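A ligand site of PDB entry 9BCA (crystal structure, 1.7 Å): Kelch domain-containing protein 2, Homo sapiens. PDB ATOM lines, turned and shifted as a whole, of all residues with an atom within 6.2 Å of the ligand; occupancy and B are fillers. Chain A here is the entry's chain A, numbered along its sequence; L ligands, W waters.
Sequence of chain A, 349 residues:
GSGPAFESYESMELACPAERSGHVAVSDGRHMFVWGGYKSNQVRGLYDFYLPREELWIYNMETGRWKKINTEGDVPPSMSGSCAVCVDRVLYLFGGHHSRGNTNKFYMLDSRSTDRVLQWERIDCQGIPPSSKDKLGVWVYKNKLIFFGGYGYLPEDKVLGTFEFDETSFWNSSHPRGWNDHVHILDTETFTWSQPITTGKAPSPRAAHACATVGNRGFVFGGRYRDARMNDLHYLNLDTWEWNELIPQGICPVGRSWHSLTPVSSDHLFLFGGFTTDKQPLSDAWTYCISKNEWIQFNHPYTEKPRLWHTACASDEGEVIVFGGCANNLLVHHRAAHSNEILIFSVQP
Residues that only touch the ligand: Tyr 38, Lys 135, Tyr 151, Asp 166, Ala 207, Ala 208, Trp 258, Trp 309, Leu 330 and Leu 331.
14 residues have an atom within 4 Å of the ligand: Tyr 38, Lys 135, Tyr 151, Asp 166, Trp 179, Ala 207, Ala 208, Arg 224, Arg 229, Ser 257, Trp 258, Trp 309, Leu 330 and Leu 331.
Water W2 lies within hydrogen-bond range of the guanidinium group of Arg 224 (2.7 Å), the side-chain carboxylate of Asp 166 (2.7 Å) and the side-chain hydroxyl of Thr 168 (3.2 Å).
The side-chain hydroxyl (OG) of Ser 257 sits at hydrogen-bond distance from an oxygen (O2) of the ligand, at 2.6 Å.
The guanidinium group (NE) of Arg 229 lies within salt-bridge range of an oxygen (O2) of the ligand (2.8 Å).
An oxygen (O3) of the ligand is in salt-bridge range of the guanidinium group of Arg 224.
O1 of the ligand is in hydrogen-bond range of NE1 of Trp 179.
The guanidinium group (NE) of Arg 229 sits close to the side-chain hydroxyl (OG) of Ser 257 (3.4 Å).
The backbone NH (N) of Arg 224 is in hydrogen-bond range of the backbone carbonyl oxygen (O) of Ala 207 (2.7 Å).
OH of Tyr 151 lies within hydrogen-bond range of OD2 of Asp 166 (2.9 Å).
The side-chain carboxylate of Asp 166 sits at hydrogen-bond distance from the side-chain hydroxyl of Thr 168 (2.6 Å).
The backbone NH (N) of Asp 166 is in hydrogen-bond range of the backbone carbonyl oxygen (O) of Arg 177, 2.9 Å away.
N of Trp 258 lies within hydrogen-bond range of O of Ala 208 (3.0 Å).
O of Trp 258 sits at hydrogen-bond distance from N of Trp 309 (2.9 Å).
O of Lys 135 sits at hydrogen-bond distance from N of Ala 208.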
ATOM      1  N   TYR A  38     -23.245  29.581 -23.701  1.00  0.00           N
ATOM      2  CA  TYR A  38     -22.218  28.578 -23.948  1.00  0.00           C
ATOM      3  C   TYR A  38     -22.903  27.272 -24.295  1.00  0.00           C
ATOM      4  O   TYR A  38     -24.116  27.123 -24.119  1.00  0.00           O
ATOM      5  CB  TYR A  38     -21.299  28.393 -22.717  1.00  0.00           C
ATOM      6  CG  TYR A  38     -21.912  27.459 -21.686  1.00  0.00           C
ATOM      7  CD1 TYR A  38     -23.022  27.848 -20.933  1.00  0.00           C
ATOM      8  CD2 TYR A  38     -21.395  26.193 -21.478  1.00  0.00           C
ATOM      9  CE1 TYR A  38     -23.591  26.987 -19.988  1.00  0.00           C
ATOM     10  CE2 TYR A  38     -21.956  25.334 -20.537  1.00  0.00           C
ATOM     11  CZ  TYR A  38     -23.052  25.725 -19.803  1.00  0.00           C
ATOM     12  OH  TYR A  38     -23.616  24.873 -18.886  1.00  0.00           O
ATOM     13  N   LYS A 135     -25.464  35.658 -13.362  1.00  0.00           N
ATOM     14  CA  LYS A 135     -26.627  34.917 -12.876  1.00  0.00           C
ATOM     15  C   LYS A 135     -27.418  35.718 -11.837  1.00  0.00           C
ATOM     16  O   LYS A 135     -27.634  35.297 -10.698  1.00  0.00           O
ATOM     17  CB  LYS A 135     -26.201  33.559 -12.314  1.00  0.00           C
ATOM     18  CG  LYS A 135     -25.583  32.609 -13.345  1.00  0.00           C
ATOM     19  CD  LYS A 135     -25.331  31.209 -12.756  1.00  0.00           C
ATOM     20  CE  LYS A 135     -24.157  31.171 -11.790  1.00  0.00           C
ATOM     21  NZ  LYS A 135     -22.926  31.513 -12.526  1.00  0.00           N
ATOM     22  N   TYR A 151     -23.821  36.018  -8.626  1.00  0.00           N
ATOM     23  CA  TYR A 151     -22.650  35.228  -8.232  1.00  0.00           C
ATOM     24  C   TYR A 151     -21.402  35.899  -8.798  1.00  0.00           C
ATOM     25  O   TYR A 151     -21.364  36.160 -10.003  1.00  0.00           O
ATOM     26  CB  TYR A 151     -22.753  33.828  -8.794  1.00  0.00           C
ATOM     27  CG  TYR A 151     -21.779  32.800  -8.230  1.00  0.00           C
ATOM     28  CD1 TYR A 151     -21.857  32.388  -6.898  1.00  0.00           C
ATOM     29  CD2 TYR A 151     -20.811  32.199  -9.042  1.00  0.00           C
ATOM     30  CE1 TYR A 151     -20.995  31.429  -6.389  1.00  0.00           C
ATOM     31  CE2 TYR A 151     -19.952  31.219  -8.526  1.00  0.00           C
ATOM     32  CZ  TYR A 151     -20.043  30.855  -7.200  1.00  0.00           C
ATOM     33  OH  TYR A 151     -19.199  29.914  -6.675  1.00  0.00           O
ATOM     34  N   ASP A 166     -19.135  31.176  -1.511  1.00  0.00           N
ATOM     35  CA  ASP A 166     -19.426  29.779  -1.822  1.00  0.00           C
ATOM     36  C   ASP A 166     -18.164  28.967  -1.546  1.00  0.00           C
ATOM     37  O   ASP A 166     -17.184  29.045  -2.287  1.00  0.00           O
ATOM     38  CB  ASP A 166     -19.872  29.632  -3.280  1.00  0.00           C
ATOM     39  CG  ASP A 166     -20.098  28.185  -3.701  1.00  0.00           C
ATOM     40  OD1 ASP A 166     -19.923  27.254  -2.874  1.00  0.00           O
ATOM     41  OD2 ASP A 166     -20.431  27.989  -4.881  1.00  0.00           O
ATOM     42  N   THR A 168     -17.317  26.004  -2.014  1.00  0.00           N
ATOM     43  CA  THR A 168     -16.876  25.108  -3.075  1.00  0.00           C
ATOM     44  C   THR A 168     -15.955  25.783  -4.076  1.00  0.00           C
ATOM     45  O   THR A 168     -15.319  25.075  -4.880  1.00  0.00           O
ATOM     46  CB  THR A 168     -18.069  24.512  -3.834  1.00  0.00           C
ATOM     47  OG1 THR A 168     -18.797  25.560  -4.489  1.00  0.00           O
ATOM     48  CG2 THR A 168     -18.982  23.724  -2.922  1.00  0.00           C
ATOM     49  N   ARG A 177     -15.498  32.926  -5.021  1.00  0.00           N
ATOM     50  CA  ARG A 177     -16.690  33.630  -5.463  1.00  0.00           C
ATOM     51  C   ARG A 177     -17.838  33.327  -4.515  1.00  0.00           C
ATOM     52  O   ARG A 177     -17.799  32.364  -3.739  1.00  0.00           O
ATOM     53  CB  ARG A 177     -17.044  33.269  -6.911  1.00  0.00           C
ATOM     54  CG  ARG A 177     -15.917  33.592  -7.911  1.00  0.00           C
ATOM     55  CD  ARG A 177     -16.324  33.435  -9.363  1.00  0.00           C
ATOM     56  NE  ARG A 177     -16.737  32.079  -9.671  1.00  0.00           N
ATOM     57  CZ  ARG A 177     -17.289  31.714 -10.826  1.00  0.00           C
ATOM     58  NH1 ARG A 177     -17.450  32.587 -11.817  1.00  0.00           N
ATOM     59  NH2 ARG A 177     -17.710  30.459 -10.984  1.00  0.00           N
ATOM     60  N   TRP A 179     -22.260  34.678  -3.323  1.00  0.00           N
ATOM     61  CA  TRP A 179     -23.560  35.249  -3.609  1.00  0.00           C
ATOM     62  C   TRP A 179     -23.727  36.599  -2.902  1.00  0.00           C
ATOM     63  O   TRP A 179     -23.193  36.815  -1.813  1.00  0.00           O
ATOM     64  CB  TRP A 179     -24.686  34.306  -3.147  1.00  0.00           C
ATOM     65  CG  TRP A 179     -24.581  32.908  -3.708  1.00  0.00           C
ATOM     66  CD1 TRP A 179     -25.051  32.483  -4.924  1.00  0.00           C
ATOM     67  CD2 TRP A 179     -24.016  31.752  -3.072  1.00  0.00           C
ATOM     68  NE1 TRP A 179     -24.781  31.148  -5.091  1.00  0.00           N
ATOM     69  CE2 TRP A 179     -24.161  30.674  -3.959  1.00  0.00           C
ATOM     70  CE3 TRP A 179     -23.400  31.540  -1.834  1.00  0.00           C
ATOM     71  CZ2 TRP A 179     -23.707  29.393  -3.659  1.00  0.00           C
ATOM     72  CZ3 TRP A 179     -22.944  30.250  -1.533  1.00  0.00           C
ATOM     73  CH2 TRP A 179     -23.116  29.204  -2.438  1.00  0.00           C
ATOM     74  N   ARG A 206     -28.312  35.436  -3.271  1.00  0.00           N
ATOM     75  CA  ARG A 206     -28.651  34.329  -4.147  1.00  0.00           C
ATOM     76  C   ARG A 206     -28.224  34.633  -5.576  1.00  0.00           C
ATOM     77  O   ARG A 206     -28.046  35.796  -5.962  1.00  0.00           O
ATOM     78  CB  ARG A 206     -30.146  34.036  -4.117  1.00  0.00           C
ATOM     79  CG  ARG A 206     -31.021  35.249  -4.410  1.00  0.00           C
ATOM     80  CD  ARG A 206     -32.493  34.943  -4.044  1.00  0.00           C
ATOM     81  NE  ARG A 206     -32.686  34.805  -2.612  1.00  0.00           N
ATOM     82  CZ  ARG A 206     -33.715  34.178  -2.073  1.00  0.00           C
ATOM     83  NH1 ARG A 206     -34.658  33.616  -2.827  1.00  0.00           N
ATOM     84  NH2 ARG A 206     -33.788  34.068  -0.752  1.00  0.00           N
ATOM     85  N   ALA A 207     -28.142  33.564  -6.360  1.00  0.00           N
ATOM     86  CA  ALA A 207     -27.915  33.638  -7.793  1.00  0.00           C
ATOM     87  C   ALA A 207     -28.838  32.660  -8.507  1.00  0.00           C
ATOM     88  O   ALA A 207     -29.347  31.707  -7.911  1.00  0.00           O
ATOM     89  CB  ALA A 207     -26.444  33.342  -8.141  1.00  0.00           C
ATOM     90  N   ALA A 208     -29.042  32.898  -9.805  1.00  0.00           N
ATOM     91  CA  ALA A 208     -29.862  32.045 -10.647  1.00  0.00           C
ATOM     92  C   ALA A 208     -31.325  32.056 -10.173  1.00  0.00           C
ATOM     93  O   ALA A 208     -32.084  31.116 -10.440  1.00  0.00           O
ATOM     94  CB  ALA A 208     -29.330  30.603 -10.710  1.00  0.00           C
ATOM     95  N   GLY A 223     -33.885  30.747  -6.561  1.00  0.00           N
ATOM     96  CA  GLY A 223     -32.461  30.982  -6.656  1.00  0.00           C
ATOM     97  C   GLY A 223     -31.665  29.972  -5.839  1.00  0.00           C
ATOM     98  O   GLY A 223     -32.197  29.183  -5.056  1.00  0.00           O
ATOM     99  N   ARG A 224     -30.351  29.997  -6.044  1.00  0.00           N
ATOM    100  CA  ARG A 224     -29.428  29.168  -5.290  1.00  0.00           C
ATOM    101  C   ARG A 224     -28.793  29.997  -4.179  1.00  0.00           C
ATOM    102  O   ARG A 224     -28.346  31.127  -4.402  1.00  0.00           O
ATOM    103  CB  ARG A 224     -28.332  28.599  -6.195  1.00  0.00           C
ATOM    104  CG  ARG A 224     -27.112  28.110  -5.433  1.00  0.00           C
ATOM    105  CD  ARG A 224     -27.209  26.636  -5.111  1.00  0.00           C
ATOM    106  NE  ARG A 224     -26.139  26.240  -4.208  1.00  0.00           N
ATOM    107  CZ  ARG A 224     -24.880  26.011  -4.584  1.00  0.00           C
ATOM    108  NH1 ARG A 224     -24.530  26.001  -5.861  1.00  0.00           N
ATOM    109  NH2 ARG A 224     -23.962  25.777  -3.648  1.00  0.00           N
ATOM    110  N   TYR A 225     -28.734  29.417  -2.974  1.00  0.00           N
ATOM    111  CA  TYR A 225     -27.980  30.016  -1.874  1.00  0.00           C
ATOM    112  C   TYR A 225     -27.499  28.916  -0.948  1.00  0.00           C
ATOM    113  O   TYR A 225     -28.317  28.166  -0.424  1.00  0.00           O
ATOM    114  CB  TYR A 225     -28.833  31.026  -1.109  1.00  0.00           C
ATOM    115  CG  TYR A 225     -28.160  31.630   0.120  1.00  0.00           C
ATOM    116  CD1 TYR A 225     -26.868  32.116   0.060  1.00  0.00           C
ATOM    117  CD2 TYR A 225     -28.842  31.721   1.323  1.00  0.00           C
ATOM    118  CE1 TYR A 225     -26.252  32.679   1.168  1.00  0.00           C
ATOM    119  CE2 TYR A 225     -28.239  32.283   2.449  1.00  0.00           C
ATOM    120  CZ  TYR A 225     -26.943  32.765   2.353  1.00  0.00           C
ATOM    121  OH  TYR A 225     -26.329  33.317   3.453  1.00  0.00           O
ATOM    122  N   ARG A 229     -31.686  25.241  -3.291  1.00  0.00           N
ATOM    123  CA  ARG A 229     -32.368  25.981  -4.335  1.00  0.00           C
ATOM    124  C   ARG A 229     -33.775  26.258  -3.854  1.00  0.00           C
ATOM    125  O   ARG A 229     -34.513  25.341  -3.498  1.00  0.00           O
ATOM    126  CB  ARG A 229     -32.337  25.196  -5.646  1.00  0.00           C
ATOM    127  CG  ARG A 229     -30.871  25.121  -6.139  1.00  0.00           C
ATOM    128  CD  ARG A 229     -30.610  24.328  -7.413  1.00  0.00           C
ATOM    129  NE  ARG A 229     -29.168  24.317  -7.670  1.00  0.00           N
ATOM    130  CZ  ARG A 229     -28.369  23.286  -7.432  1.00  0.00           C
ATOM    131  NH1 ARG A 229     -28.849  22.102  -7.077  1.00  0.00           N
ATOM    132  NH2 ARG A 229     -27.053  23.436  -7.567  1.00  0.00           N
ATOM    133  N   SER A 257     -33.533  26.705  -8.909  1.00  0.00           N
ATOM    134  CA  SER A 257     -32.787  27.772  -9.582  1.00  0.00           C
ATOM    135  C   SER A 257     -32.851  27.552 -11.083  1.00  0.00           C
ATOM    136  O   SER A 257     -33.322  26.514 -11.557  1.00  0.00           O
ATOM    137  CB  SER A 257     -31.326  27.814  -9.143  1.00  0.00           C
ATOM    138  OG  SER A 257     -30.675  26.651  -9.633  1.00  0.00           O
ATOM    139  N   TRP A 258     -32.345  28.535 -11.845  1.00  0.00           N
ATOM    140  CA  TRP A 258     -32.213  28.456 -13.295  1.00  0.00           C
ATOM    141  C   TRP A 258     -33.559  28.294 -14.011  1.00  0.00           C
ATOM    142  O   TRP A 258     -33.639  27.767 -15.117  1.00  0.00           O
ATOM    143  CB  TRP A 258     -31.245  27.328 -13.675  1.00  0.00           C
ATOM    144  CG  TRP A 258     -29.810  27.786 -13.672  1.00  0.00           C
ATOM    145  CD1 TRP A 258     -29.338  28.996 -14.053  1.00  0.00           C
ATOM    146  CD2 TRP A 258     -28.660  27.027 -13.241  1.00  0.00           C
ATOM    147  NE1 TRP A 258     -27.960  29.040 -13.917  1.00  0.00           N
ATOM    148  CE2 TRP A 258     -27.522  27.843 -13.425  1.00  0.00           C
ATOM    149  CE3 TRP A 258     -28.492  25.728 -12.751  1.00  0.00           C
ATOM    150  CZ2 TRP A 258     -26.228  27.407 -13.125  1.00  0.00           C
ATOM    151  CZ3 TRP A 258     -27.202  25.293 -12.437  1.00  0.00           C
ATOM    152  CH2 TRP A 258     -26.084  26.133 -12.629  1.00  0.00           C
ATOM    153  N   PHE A 275     -34.266  23.831 -11.721  1.00  0.00           N
ATOM    154  CA  PHE A 275     -33.361  22.809 -11.218  1.00  0.00           C
ATOM    155  C   PHE A 275     -33.526  22.700  -9.703  1.00  0.00           C
ATOM    156  O   PHE A 275     -33.280  23.687  -9.003  1.00  0.00           O
ATOM    157  CB  PHE A 275     -31.932  23.230 -11.580  1.00  0.00           C
ATOM    158  CG  PHE A 275     -30.913  22.160 -11.439  1.00  0.00           C
ATOM    159  CD1 PHE A 275     -31.159  20.877 -11.927  1.00  0.00           C
ATOM    160  CD2 PHE A 275     -29.676  22.440 -10.883  1.00  0.00           C
ATOM    161  CE1 PHE A 275     -30.198  19.900 -11.839  1.00  0.00           C
ATOM    162  CE2 PHE A 275     -28.704  21.458 -10.777  1.00  0.00           C
ATOM    163  CZ  PHE A 275     -28.968  20.172 -11.255  1.00  0.00           C
ATOM    164  N   TRP A 309     -31.683  27.105 -17.196  1.00  0.00           N
ATOM    165  CA  TRP A 309     -30.830  28.138 -17.788  1.00  0.00           C
ATOM    166  C   TRP A 309     -31.266  28.478 -19.203  1.00  0.00           C
ATOM    167  O   TRP A 309     -30.457  28.961 -20.009  1.00  0.00           O
ATOM    168  CB  TRP A 309     -29.347  27.750 -17.741  1.00  0.00           C
ATOM    169  CG  TRP A 309     -28.483  28.920 -17.367  1.00  0.00           C
ATOM    170  CD1 TRP A 309     -28.904  30.201 -17.157  1.00  0.00           C
ATOM    171  CD2 TRP A 309     -27.057  28.931 -17.177  1.00  0.00           C
ATOM    172  NE1 TRP A 309     -27.840  31.001 -16.821  1.00  0.00           N
ATOM    173  CE2 TRP A 309     -26.692  30.257 -16.838  1.00  0.00           C
ATOM    174  CE3 TRP A 309     -26.065  27.944 -17.227  1.00  0.00           C
ATOM    175  CZ2 TRP A 309     -25.377  30.616 -16.558  1.00  0.00           C
ATOM    176  CZ3 TRP A 309     -24.757  28.311 -16.956  1.00  0.00           C
ATOM    177  CH2 TRP A 309     -24.420  29.638 -16.628  1.00  0.00           C
ATOM    178  N   LEU A 330     -26.663  20.311 -16.248  1.00  0.00           N
ATOM    179  CA  LEU A 330     -25.577  20.892 -17.019  1.00  0.00           C
ATOM    180  C   LEU A 330     -24.251  20.864 -16.279  1.00  0.00           C
ATOM    181  O   LEU A 330     -23.197  21.060 -16.903  1.00  0.00           O
ATOM    182  CB  LEU A 330     -25.940  22.329 -17.415  1.00  0.00           C
ATOM    183  CG  LEU A 330     -26.308  23.322 -16.312  1.00  0.00           C
ATOM    184  CD1 LEU A 330     -25.084  23.961 -15.694  1.00  0.00           C
ATOM    185  CD2 LEU A 330     -27.260  24.412 -16.834  1.00  0.00           C
ATOM    186  N   LEU A 331     -24.275  20.651 -14.968  1.00  0.00           N
ATOM    187  CA  LEU A 331     -23.048  20.582 -14.191  1.00  0.00           C
ATOM    188  C   LEU A 331     -22.222  19.348 -14.531  1.00  0.00           C
ATOM    189  O   LEU A 331     -21.035  19.312 -14.224  1.00  0.00           O
ATOM    190  CB  LEU A 331     -23.366  20.617 -12.696  1.00  0.00           C
ATOM    191  CG  LEU A 331     -24.217  21.799 -12.228  1.00  0.00           C
ATOM    192  CD1 LEU A 331     -24.682  21.612 -10.786  1.00  0.00           C
ATOM    193  CD2 LEU A 331     -23.379  23.054 -12.343  1.00  0.00           C
ATOM    194  N   VAL A 332     -22.825  18.340 -15.154  1.00  0.00           N
ATOM    195  CA  VAL A 332     -22.060  17.226 -15.735  1.00  0.00           C
ATOM    196  C   VAL A 332     -21.811  17.626 -17.182  1.00  0.00           C
ATOM    197  O   VAL A 332     -22.516  17.228 -18.118  1.00  0.00           O
ATOM    198  CB  VAL A 332     -22.792  15.885 -15.605  1.00  0.00           C
ATOM    199  CG1 VAL A 332     -21.927  14.779 -16.168  1.00  0.00           C
ATOM    200  CG2 VAL A 332     -23.135  15.616 -14.157  1.00  0.00           C
ATOM    201  N   HIS A 333     -20.771  18.446 -17.376  1.00  0.00           N
ATOM    202  CA  HIS A 333     -20.652  19.193 -18.620  1.00  0.00           C
ATOM    203  C   HIS A 333     -20.478  18.261 -19.826  1.00  0.00           C
ATOM    204  O   HIS A 333     -21.009  18.536 -20.905  1.00  0.00           O
ATOM    205  CB  HIS A 333     -19.516  20.213 -18.501  1.00  0.00           C
ATOM    206  CG  HIS A 333     -19.320  21.056 -19.716  1.00  0.00           C
ATOM    207  ND1 HIS A 333     -20.186  22.063 -20.087  1.00  0.00           N
ATOM    208  CD2 HIS A 333     -18.337  21.047 -20.652  1.00  0.00           C
ATOM    209  CE1 HIS A 333     -19.742  22.641 -21.195  1.00  0.00           C
ATOM    210  NE2 HIS A 333     -18.625  22.032 -21.563  1.00  0.00           N
HETATM  211  C1  LIG L   1     -21.280  27.540  -8.282  1.00  0.00           C
HETATM  212  C2  LIG L   1     -21.624  26.410 -12.166  1.00  0.00           C
HETATM  213  C3  LIG L   1     -22.471  26.473 -14.418  1.00  0.00           C
HETATM  214  C4  LIG L   1     -21.624  24.891 -16.062  1.00  0.00           C
HETATM  215  C5  LIG L   1     -19.951  23.771 -14.149  1.00  0.00           C
HETATM  216  C6  LIG L   1     -20.791  24.845 -13.807  1.00  0.00           C
HETATM  217  C7  LIG L   1     -20.781  25.360 -12.493  1.00  0.00           C
HETATM  218  C8  LIG L   1     -24.607  29.265  -8.431  1.00  0.00           C
HETATM  219  C9  LIG L   1     -26.550  28.194  -9.660  1.00  0.00           C
HETATM  220  C10 LIG L   1     -26.952  26.910  -8.940  1.00  0.00           C
HETATM  221  C11 LIG L   1     -23.086  29.371  -8.266  1.00  0.00           C
HETATM  222  C12 LIG L   1     -22.283  28.274  -8.961  1.00  0.00           C
HETATM  223  C13 LIG L   1     -21.637  26.974 -10.749  1.00  0.00           C
HETATM  224  C14 LIG L   1     -22.475  26.972 -13.115  1.00  0.00           C
HETATM  225  C15 LIG L   1     -21.618  25.403 -14.756  1.00  0.00           C
HETATM  226  C16 LIG L   1     -20.789  23.836 -16.406  1.00  0.00           C
HETATM  227  C17 LIG L   1     -19.953  23.261 -15.446  1.00  0.00           C
HETATM  228  N1  LIG L   1     -25.120  28.366  -9.446  1.00  0.00           N
HETATM  229  N2  LIG L   1     -22.432  27.941 -10.276  1.00  0.00           N
HETATM  230  O1  LIG L   1     -25.313  29.928  -7.752  1.00  0.00           O
HETATM  231  O2  LIG L   1     -28.154  26.532  -8.952  1.00  0.00           O
HETATM  232  O3  LIG L   1     -26.080  26.226  -8.336  1.00  0.00           O
HETATM  233  S1  LIG L   1     -20.650  26.492  -9.453  1.00  0.00           S
HETATM  234  O   HOH W   1     -23.772  25.196  -9.294  1.00  0.00           O
HETATM  235  O   HOH W   2     -21.855  25.741  -5.459  1.00  0.00           O
HETATM  236  O   HOH W   3     -19.156  20.853 -12.774  1.00  0.00           O
